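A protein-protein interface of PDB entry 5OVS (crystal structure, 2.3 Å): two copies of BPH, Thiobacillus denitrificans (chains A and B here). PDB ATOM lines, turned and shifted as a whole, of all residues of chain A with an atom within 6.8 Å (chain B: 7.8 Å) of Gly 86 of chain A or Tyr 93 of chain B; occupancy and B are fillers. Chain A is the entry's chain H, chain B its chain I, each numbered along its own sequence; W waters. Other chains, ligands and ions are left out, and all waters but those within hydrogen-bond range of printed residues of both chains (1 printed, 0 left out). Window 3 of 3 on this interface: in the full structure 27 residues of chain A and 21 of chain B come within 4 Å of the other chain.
ND2 of Asn 82 of chain A touches CD1 of Tyr 92 of chain B, 3.6 Å away.
Asn 82 of chain A touches Tyr 93 of chain B.
His 85 of chain A touches Tyr 93 of chain B (CD2 to CG, 3.5 Å).
Tyr 93 of chain B touches Lys 89 of chain A (CD1 to NZ, 3.97 Å).
Asp 103 of chain A touches Leu 94 of chain B.
Leu 104 of chain A touches Tyr 92 of chain B.
Tyr 93 of chain B touches Leu 104 of chain A.
Leu 104 of chain A touches Gln 95 of chain B (C to CG, 3.8 Å).
Gln 95 of chain B touches Glu 105 of chain A.
Tyr 93 of chain B touches Arg 126 of chain A.
Of chain B, only Tyr 93 (3.1 Å) comes within 4 Å of Gly 86 of chain A.
Of the printed residues of chain B, Lys 89 of chain A touches Tyr 93 (3.97 Å).
Printed residues of chain B within 4 Å of Glu 105 of chain A: Tyr 93 and Gln 95.
Tyr 93 of chain B touches just these residues of chain A: Asn 82, His 85, Gly 86, Lys 89, Leu 104, Glu 105 and Arg 126.
The nearest residue of chain B that does not touch Gly 86 of chain A is His 91 of chain B (7.3 Å).
The nearest residue of chain A that does not touch Tyr 93 of chain B is Asp 103 of chain A (4.6 Å).
NE2 of His 85 of chain A is in hydrogen-bond range of OE1 of Glu 105 of chain A, 3.2 Å away.
ND1 of His 85 of chain A sits at hydrogen-bond distance from OG of Ser 107 of chain A (2.6 Å).
NZ of Lys 89 of chain A lies within salt-bridge range of OE1 of Glu 105 of chain A, 2.8 Å away.
The backbone NH of Tyr 92 of chain B lies close to the backbone carbonyl oxygen of Ala 87 of chain B, 3.5 Å away.
The backbone carbonyl oxygen of Leu 88 of chain B sits at hydrogen-bond distance from the backbone NH of Tyr 93 of chain B, 3.2 Å away.
The backbone carbonyl oxygen (O) of Leu 88 of chain B lies within hydrogen-bond range of the backbone NH (N) of Leu 94 of chain B (3.2 Å).
Hydrophobic or aromatic side chains of chain A that line the printed part of chain B: His 85 and Leu 104.
Of the 10 printed residues of chain B, 5 touch a printed residue of chain A.
5 positions are printed for both chains.
Of the 14 pairs that touch across the chains among the printed residues, none has its exchanged pair printed and touching as well.
ND2 of Asn 82 of chain A lies within hydrogen-bond range of O of His 91 of chain B (2.9 Å).
The side-chain hydroxyl (OH) of Tyr 93 of chain B lies close to the backbone NH (N) of Gly 86 of chain A (3.3 Å).
The backbone NH (N) of Gln 95 of chain B lies within hydrogen-bond range of the backbone carbonyl oxygen (O) of Asp 103 of chain A (3.2 Å).
The backbone NH (N) of Glu 105 of chain A is in hydrogen-bond range of the backbone carbonyl oxygen (O) of Tyr 93 of chain B (2.9 Å).
Water W1 lies within hydrogen-bond range of O of Tyr 92 of chain B (2.7 Å), NE of Arg 126 of chain A (2.8 Å) and OD1 of Asn 82 of chain A (3.0 Å).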
ATOM      1  N   TRP A  81       5.776   9.341  19.055  1.00  0.00           N
ATOM      2  CA  TRP A  81       4.453   8.721  18.901  1.00  0.00           C
ATOM      3  C   TRP A  81       3.650   8.675  20.193  1.00  0.00           C
ATOM      4  O   TRP A  81       2.432   8.837  20.172  1.00  0.00           O
ATOM      5  CB  TRP A  81       4.546   7.310  18.309  1.00  0.00           C
ATOM      6  CG  TRP A  81       3.982   7.230  16.935  1.00  0.00           C
ATOM      7  CD1 TRP A  81       2.898   6.500  16.529  1.00  0.00           C
ATOM      8  CD2 TRP A  81       4.461   7.918  15.776  1.00  0.00           C
ATOM      9  NE1 TRP A  81       2.685   6.678  15.180  1.00  0.00           N
ATOM     10  CE2 TRP A  81       3.628   7.545  14.694  1.00  0.00           C
ATOM     11  CE3 TRP A  81       5.519   8.805  15.543  1.00  0.00           C
ATOM     12  CZ2 TRP A  81       3.812   8.045  13.407  1.00  0.00           C
ATOM     13  CZ3 TRP A  81       5.707   9.295  14.261  1.00  0.00           C
ATOM     14  CH2 TRP A  81       4.853   8.910  13.207  1.00  0.00           C
ATOM     15  N   ASN A  82       4.317   8.433  21.314  1.00  0.00           N
ATOM     16  CA  ASN A  82       3.631   8.447  22.596  1.00  0.00           C
ATOM     17  C   ASN A  82       2.950   9.795  22.800  1.00  0.00           C
ATOM     18  O   ASN A  82       1.768   9.849  23.135  1.00  0.00           O
ATOM     19  CB  ASN A  82       4.587   8.139  23.751  1.00  0.00           C
ATOM     20  CG  ASN A  82       3.851   7.783  25.025  1.00  0.00           C
ATOM     21  OD1 ASN A  82       3.075   6.829  25.051  1.00  0.00           O
ATOM     22  ND2 ASN A  82       4.084   8.548  26.088  1.00  0.00           N
ATOM     23  N   THR A  83       3.689  10.874  22.560  1.00  0.00           N
ATOM     24  CA  THR A  83       3.149  12.229  22.697  1.00  0.00           C
ATOM     25  C   THR A  83       2.085  12.522  21.639  1.00  0.00           C
ATOM     26  O   THR A  83       1.086  13.179  21.927  1.00  0.00           O
ATOM     27  CB  THR A  83       4.271  13.281  22.609  1.00  0.00           C
ATOM     28  OG1 THR A  83       5.235  13.018  23.634  1.00  0.00           O
ATOM     29  CG2 THR A  83       3.726  14.693  22.784  1.00  0.00           C
ATOM     30  N   LEU A  84       2.307  12.034  20.420  1.00  0.00           N
ATOM     31  CA  LEU A  84       1.299  12.111  19.353  1.00  0.00           C
ATOM     32  C   LEU A  84      -0.053  11.541  19.784  1.00  0.00           C
ATOM     33  O   LEU A  84      -1.106  12.119  19.501  1.00  0.00           O
ATOM     34  CB  LEU A  84       1.776  11.364  18.102  1.00  0.00           C
ATOM     35  CG  LEU A  84       0.736  11.151  16.999  1.00  0.00           C
ATOM     36  CD1 LEU A  84       0.289  12.490  16.449  1.00  0.00           C
ATOM     37  CD2 LEU A  84       1.270  10.279  15.880  1.00  0.00           C
ATOM     38  N   HIS A  85      -0.019  10.401  20.459  1.00  0.00           N
ATOM     39  CA  HIS A  85      -1.247   9.725  20.867  1.00  0.00           C
ATOM     40  C   HIS A  85      -2.078  10.595  21.810  1.00  0.00           C
ATOM     41  O   HIS A  85      -3.295  10.692  21.653  1.00  0.00           O
ATOM     42  CB  HIS A  85      -0.931   8.379  21.504  1.00  0.00           C
ATOM     43  CG  HIS A  85      -2.151   7.628  21.919  1.00  0.00           C
ATOM     44  ND1 HIS A  85      -2.902   6.882  21.038  1.00  0.00           N
ATOM     45  CD2 HIS A  85      -2.769   7.531  23.119  1.00  0.00           C
ATOM     46  CE1 HIS A  85      -3.928   6.355  21.679  1.00  0.00           C
ATOM     47  NE2 HIS A  85      -3.872   6.734  22.942  1.00  0.00           N
ATOM     48  N   GLY A  86      -1.404  11.251  22.759  1.00  0.00           N
ATOM     49  CA  GLY A  86      -2.027  12.245  23.644  1.00  0.00           C
ATOM     50  C   GLY A  86      -2.724  13.379  22.910  1.00  0.00           C
ATOM     51  O   GLY A  86      -3.741  13.909  23.380  1.00  0.00           O
ATOM     52  N   ALA A  87      -2.168  13.757  21.761  1.00  0.00           N
ATOM     53  CA  ALA A  87      -2.738  14.797  20.919  1.00  0.00           C
ATOM     54  C   ALA A  87      -3.870  14.271  20.035  1.00  0.00           C
ATOM     55  O   ALA A  87      -4.847  14.979  19.805  1.00  0.00           O
ATOM     56  CB  ALA A  87      -1.649  15.419  20.061  1.00  0.00           C
ATOM     57  N   LEU A  88      -3.746  13.045  19.524  1.00  0.00           N
ATOM     58  CA  LEU A  88      -4.838  12.450  18.762  1.00  0.00           C
ATOM     59  C   LEU A  88      -6.123  12.450  19.600  1.00  0.00           C
ATOM     60  O   LEU A  88      -7.211  12.714  19.094  1.00  0.00           O
ATOM     61  CB  LEU A  88      -4.501  11.016  18.326  1.00  0.00           C
ATOM     62  CG  LEU A  88      -3.358  10.836  17.316  1.00  0.00           C
ATOM     63  CD1 LEU A  88      -3.076   9.366  17.059  1.00  0.00           C
ATOM     64  CD2 LEU A  88      -3.661  11.546  16.011  1.00  0.00           C
ATOM     65  N   LYS A  89      -5.982  12.156  20.887  1.00  0.00           N
ATOM     66  CA  LYS A  89      -7.117  12.100  21.789  1.00  0.00           C
ATOM     67  C   LYS A  89      -7.652  13.482  22.127  1.00  0.00           C
ATOM     68  O   LYS A  89      -8.862  13.713  22.079  1.00  0.00           O
ATOM     69  CB  LYS A  89      -6.716  11.401  23.084  1.00  0.00           C
ATOM     70  CG  LYS A  89      -6.394   9.927  22.916  1.00  0.00           C
ATOM     71  CD  LYS A  89      -5.833   9.358  24.206  1.00  0.00           C
ATOM     72  CE  LYS A  89      -6.893   9.244  25.285  1.00  0.00           C
ATOM     73  NZ  LYS A  89      -6.307   8.701  26.541  1.00  0.00           N
ATOM     74  N   GLU A  90      -6.742  14.385  22.483  1.00  0.00           N
ATOM     75  CA  GLU A  90      -7.109  15.685  23.036  1.00  0.00           C
ATOM     76  C   GLU A  90      -7.611  16.671  21.974  1.00  0.00           C
ATOM     77  O   GLU A  90      -8.598  17.361  22.218  1.00  0.00           O
ATOM     78  CB  GLU A  90      -5.935  16.283  23.827  1.00  0.00           C
ATOM     79  CG  GLU A  90      -6.268  17.596  24.534  1.00  0.00           C
ATOM     80  CD  GLU A  90      -5.313  17.954  25.671  1.00  0.00           C
ATOM     81  OE1 GLU A  90      -4.120  17.573  25.630  1.00  0.00           O
ATOM     82  OE2 GLU A  90      -5.764  18.635  26.618  1.00  0.00           O
ATOM     83  N   HIS A  91      -6.954  16.722  20.808  1.00  0.00           N
ATOM     84  CA  HIS A  91      -7.253  17.723  19.762  1.00  0.00           C
ATOM     85  C   HIS A  91      -7.927  17.196  18.479  1.00  0.00           C
ATOM     86  O   HIS A  91      -8.462  17.998  17.716  1.00  0.00           O
ATOM     87  CB  HIS A  91      -5.974  18.468  19.360  1.00  0.00           C
ATOM     88  CG  HIS A  91      -5.235  19.070  20.519  1.00  0.00           C
ATOM     89  ND1 HIS A  91      -5.734  20.123  21.259  1.00  0.00           N
ATOM     90  CD2 HIS A  91      -4.035  18.759  21.068  1.00  0.00           C
ATOM     91  CE1 HIS A  91      -4.877  20.432  22.217  1.00  0.00           C
ATOM     92  NE2 HIS A  91      -3.839  19.618  22.124  1.00  0.00           N
ATOM     93  N   ASP A 103      -3.918  -4.247  25.870  1.00  0.00           N
ATOM     94  CA  ASP A 103      -2.998  -3.810  26.937  1.00  0.00           C
ATOM     95  C   ASP A 103      -2.910  -2.290  27.037  1.00  0.00           C
ATOM     96  O   ASP A 103      -3.093  -1.703  28.101  1.00  0.00           O
ATOM     97  CB  ASP A 103      -1.581  -4.346  26.688  1.00  0.00           C
ATOM     98  CG  ASP A 103      -1.482  -5.853  26.827  1.00  0.00           C
ATOM     99  OD1 ASP A 103      -2.532  -6.511  27.020  1.00  0.00           O
ATOM    100  OD2 ASP A 103      -0.341  -6.375  26.745  1.00  0.00           O
ATOM    101  N   LEU A 104      -2.613  -1.672  25.900  1.00  0.00           N
ATOM    102  CA  LEU A 104      -2.461  -0.231  25.786  1.00  0.00           C
ATOM    103  C   LEU A 104      -3.552   0.324  24.876  1.00  0.00           C
ATOM    104  O   LEU A 104      -4.140  -0.409  24.054  1.00  0.00           O
ATOM    105  CB  LEU A 104      -1.087   0.079  25.191  1.00  0.00           C
ATOM    106  CG  LEU A 104       0.084  -0.580  25.925  1.00  0.00           C
ATOM    107  CD1 LEU A 104       1.323  -0.608  25.046  1.00  0.00           C
ATOM    108  CD2 LEU A 104       0.370   0.139  27.236  1.00  0.00           C
ATOM    109  N   GLU A 105      -3.820   1.619  25.011  1.00  0.00           N
ATOM    110  CA  GLU A 105      -4.731   2.278  24.084  1.00  0.00           C
ATOM    111  C   GLU A 105      -4.166   2.218  22.674  1.00  0.00           C
ATOM    112  O   GLU A 105      -2.954   2.219  22.479  1.00  0.00           O
ATOM    113  CB  GLU A 105      -4.985   3.729  24.490  1.00  0.00           C
ATOM    114  CG  GLU A 105      -5.844   3.858  25.739  1.00  0.00           C
ATOM    115  CD  GLU A 105      -5.977   5.284  26.228  1.00  0.00           C
ATOM    116  OE1 GLU A 105      -5.782   6.226  25.437  1.00  0.00           O
ATOM    117  OE2 GLU A 105      -6.284   5.460  27.420  1.00  0.00           O
ATOM    118  N   SER A 106      -5.058   2.139  21.699  1.00  0.00           N
ATOM    119  CA  SER A 106      -4.664   2.105  20.303  1.00  0.00           C
ATOM    120  C   SER A 106      -4.653   3.517  19.726  1.00  0.00           C
ATOM    121  O   SER A 106      -5.490   4.348  20.059  1.00  0.00           O
ATOM    122  CB  SER A 106      -5.593   1.194  19.481  1.00  0.00           C
ATOM    123  OG  SER A 106      -5.228   1.210  18.104  1.00  0.00           O
ATOM    124  N   SER A 107      -3.671   3.771  18.869  1.00  0.00           N
ATOM    125  CA  SER A 107      -3.620   4.981  18.071  1.00  0.00           C
ATOM    126  C   SER A 107      -4.363   4.789  16.745  1.00  0.00           C
ATOM    127  O   SER A 107      -4.606   5.765  16.033  1.00  0.00           O
ATOM    128  CB  SER A 107      -2.164   5.393  17.847  1.00  0.00           C
ATOM    129  OG  SER A 107      -1.560   5.735  19.091  1.00  0.00           O
ATOM    130  N   ARG A 126       1.821   1.644  19.576  1.00  0.00           N
ATOM    131  CA  ARG A 126       3.097   2.355  19.767  1.00  0.00           C
ATOM    132  C   ARG A 126       4.319   1.448  19.840  1.00  0.00           C
ATOM    133  O   ARG A 126       5.365   1.815  20.393  1.00  0.00           O
ATOM    134  CB  ARG A 126       3.012   3.348  20.938  1.00  0.00           C
ATOM    135  CG  ARG A 126       2.181   4.568  20.540  1.00  0.00           C
ATOM    136  CD  ARG A 126       1.598   5.366  21.698  1.00  0.00           C
ATOM    137  NE  ARG A 126       0.907   4.550  22.692  1.00  0.00           N
ATOM    138  CZ  ARG A 126      -0.251   3.908  22.507  1.00  0.00           C
ATOM    139  NH1 ARG A 126      -0.898   3.949  21.338  1.00  0.00           N
ATOM    140  NH2 ARG A 126      -0.758   3.199  23.515  1.00  0.00           N
ATOM    141  N   ILE B  57       8.553   1.470  26.789  1.00  0.00           N
ATOM    142  CA  ILE B  57       7.965   2.241  27.872  1.00  0.00           C
ATOM    143  C   ILE B  57       8.893   2.234  29.092  1.00  0.00           C
ATOM    144  O   ILE B  57       9.257   3.306  29.600  1.00  0.00           O
ATOM    145  CB  ILE B  57       6.553   1.704  28.233  1.00  0.00           C
ATOM    146  CG1 ILE B  57       5.546   2.101  27.155  1.00  0.00           C
ATOM    147  CG2 ILE B  57       6.093   2.219  29.600  1.00  0.00           C
ATOM    148  CD1 ILE B  57       4.196   1.435  27.308  1.00  0.00           C
ATOM    149  N   ALA B  87       2.531   5.519  36.478  1.00  0.00           N
ATOM    150  CA  ALA B  87       3.077   6.140  35.262  1.00  0.00           C
ATOM    151  C   ALA B  87       2.588   5.462  33.981  1.00  0.00           C
ATOM    152  O   ALA B  87       2.439   6.125  32.953  1.00  0.00           O
ATOM    153  CB  ALA B  87       4.593   6.134  35.297  1.00  0.00           C
ATOM    154  N   LEU B  88       2.373   4.150  34.032  1.00  0.00           N
ATOM    155  CA  LEU B  88       1.798   3.424  32.901  1.00  0.00           C
ATOM    156  C   LEU B  88       0.446   4.023  32.536  1.00  0.00           C
ATOM    157  O   LEU B  88       0.234   4.432  31.409  1.00  0.00           O
ATOM    158  CB  LEU B  88       1.636   1.944  33.232  1.00  0.00           C
ATOM    159  CG  LEU B  88       2.920   1.130  33.398  1.00  0.00           C
ATOM    160  CD1 LEU B  88       2.605  -0.319  33.710  1.00  0.00           C
ATOM    161  CD2 LEU B  88       3.797   1.227  32.153  1.00  0.00           C
ATOM    162  N   LYS B  89      -0.447   4.112  33.510  1.00  0.00           N
ATOM    163  CA  LYS B  89      -1.769   4.699  33.291  1.00  0.00           C
ATOM    164  C   LYS B  89      -1.726   6.155  32.850  1.00  0.00           C
ATOM    165  O   LYS B  89      -2.483   6.563  31.972  1.00  0.00           O
ATOM    166  CB  LYS B  89      -2.594   4.621  34.562  1.00  0.00           C
ATOM    167  CG  LYS B  89      -2.978   3.209  34.935  1.00  0.00           C
ATOM    168  CD  LYS B  89      -3.565   3.156  36.326  1.00  0.00           C
ATOM    169  CE  LYS B  89      -5.000   3.658  36.361  1.00  0.00           C
ATOM    170  NZ  LYS B  89      -5.470   3.808  37.765  1.00  0.00           N
ATOM    171  N   GLU B  90      -0.851   6.938  33.468  1.00  0.00           N
ATOM    172  CA  GLU B  90      -0.891   8.385  33.307  1.00  0.00           C
ATOM    173  C   GLU B  90      -0.190   8.879  32.038  1.00  0.00           C
ATOM    174  O   GLU B  90      -0.729   9.732  31.344  1.00  0.00           O
ATOM    175  CB  GLU B  90      -0.310   9.056  34.552  1.00  0.00           C
ATOM    176  CG  GLU B  90      -0.635  10.538  34.681  1.00  0.00           C
ATOM    177  CD  GLU B  90      -0.362  11.073  36.076  1.00  0.00           C
ATOM    178  OE1 GLU B  90      -0.789  10.422  37.063  1.00  0.00           O
ATOM    179  OE2 GLU B  90       0.277  12.148  36.189  1.00  0.00           O
ATOM    180  N   HIS B  91       0.990   8.346  31.725  1.00  0.00           N
ATOM    181  CA  HIS B  91       1.793   8.863  30.610  1.00  0.00           C
ATOM    182  C   HIS B  91       1.901   7.916  29.431  1.00  0.00           C
ATOM    183  O   HIS B  91       2.329   8.337  28.368  1.00  0.00           O
ATOM    184  CB  HIS B  91       3.209   9.192  31.071  1.00  0.00           C
ATOM    185  CG  HIS B  91       3.269  10.024  32.314  1.00  0.00           C
ATOM    186  ND1 HIS B  91       2.939  11.363  32.331  1.00  0.00           N
ATOM    187  CD2 HIS B  91       3.635   9.711  33.580  1.00  0.00           C
ATOM    188  CE1 HIS B  91       3.086  11.835  33.556  1.00  0.00           C
ATOM    189  NE2 HIS B  91       3.511  10.855  34.333  1.00  0.00           N
ATOM    190  N   TYR B  92       1.549   6.646  29.609  1.00  0.00           N
ATOM    191  CA  TYR B  92       1.774   5.641  28.567  1.00  0.00           C
ATOM    192  C   TYR B  92       0.513   4.951  28.075  1.00  0.00           C
ATOM    193  O   TYR B  92       0.592   4.012  27.291  1.00  0.00           O
ATOM    194  CB  TYR B  92       2.805   4.606  29.047  1.00  0.00           C
ATOM    195  CG  TYR B  92       4.160   5.221  29.281  1.00  0.00           C
ATOM    196  CD1 TYR B  92       4.889   5.749  28.222  1.00  0.00           C
ATOM    197  CD2 TYR B  92       4.693   5.321  30.560  1.00  0.00           C
ATOM    198  CE1 TYR B  92       6.121   6.338  28.423  1.00  0.00           C
ATOM    199  CE2 TYR B  92       5.927   5.909  30.770  1.00  0.00           C
ATOM    200  CZ  TYR B  92       6.632   6.414  29.696  1.00  0.00           C
ATOM    201  OH  TYR B  92       7.846   7.003  29.892  1.00  0.00           O
ATOM    202  N   TYR B  93      -0.643   5.434  28.525  1.00  0.00           N
ATOM    203  CA  TYR B  93      -1.950   5.019  28.001  1.00  0.00           C
ATOM    204  C   TYR B  93      -2.265   3.547  28.263  1.00  0.00           C
ATOM    205  O   TYR B  93      -2.859   2.860  27.423  1.00  0.00           O
ATOM    206  CB  TYR B  93      -2.051   5.387  26.515  1.00  0.00           C
ATOM    207  CG  TYR B  93      -1.631   6.817  26.313  1.00  0.00           C
ATOM    208  CD1 TYR B  93      -2.434   7.856  26.771  1.00  0.00           C
ATOM    209  CD2 TYR B  93      -0.410   7.134  25.737  1.00  0.00           C
ATOM    210  CE1 TYR B  93      -2.051   9.174  26.625  1.00  0.00           C
ATOM    211  CE2 TYR B  93      -0.020   8.454  25.588  1.00  0.00           C
ATOM    212  CZ  TYR B  93      -0.846   9.465  26.037  1.00  0.00           C
ATOM    213  OH  TYR B  93      -0.476  10.777  25.904  1.00  0.00           O
ATOM    214  N   LEU B  94      -1.869   3.077  29.447  1.00  0.00           N
ATOM    215  CA  LEU B  94      -2.255   1.755  29.898  1.00  0.00           C
ATOM    216  C   LEU B  94      -3.759   1.756  30.119  1.00  0.00           C
ATOM    217  O   LEU B  94      -4.305   2.763  30.565  1.00  0.00           O
ATOM    218  CB  LEU B  94      -1.549   1.392  31.202  1.00  0.00           C
ATOM    219  CG  LEU B  94      -1.812  -0.046  31.678  1.00  0.00           C
ATOM    220  CD1 LEU B  94      -1.115  -1.057  30.777  1.00  0.00           C
ATOM    221  CD2 LEU B  94      -1.379  -0.242  33.122  1.00  0.00           C
ATOM    222  N   GLN B  95      -4.415   0.634  29.813  1.00  0.00           N
ATOM    223  CA  GLN B  95      -5.867   0.494  29.999  1.00  0.00           C
ATOM    224  C   GLN B  95      -6.280  -0.148  31.334  1.00  0.00           C
ATOM    225  O   GLN B  95      -5.708  -1.148  31.759  1.00  0.00           O
ATOM    226  CB  GLN B  95      -6.459  -0.289  28.828  1.00  0.00           C
ATOM    227  CG  GLN B  95      -6.306   0.435  27.506  1.00  0.00           C
ATOM    228  CD  GLN B  95      -7.330   0.003  26.472  1.00  0.00           C
ATOM    229  OE1 GLN B  95      -7.323  -1.144  26.018  1.00  0.00           O
ATOM    230  NE2 GLN B  95      -8.210   0.926  26.085  1.00  0.00           N
HETATM  231  O   HOH W   1       2.141   3.995  25.093  1.00  0.00           O
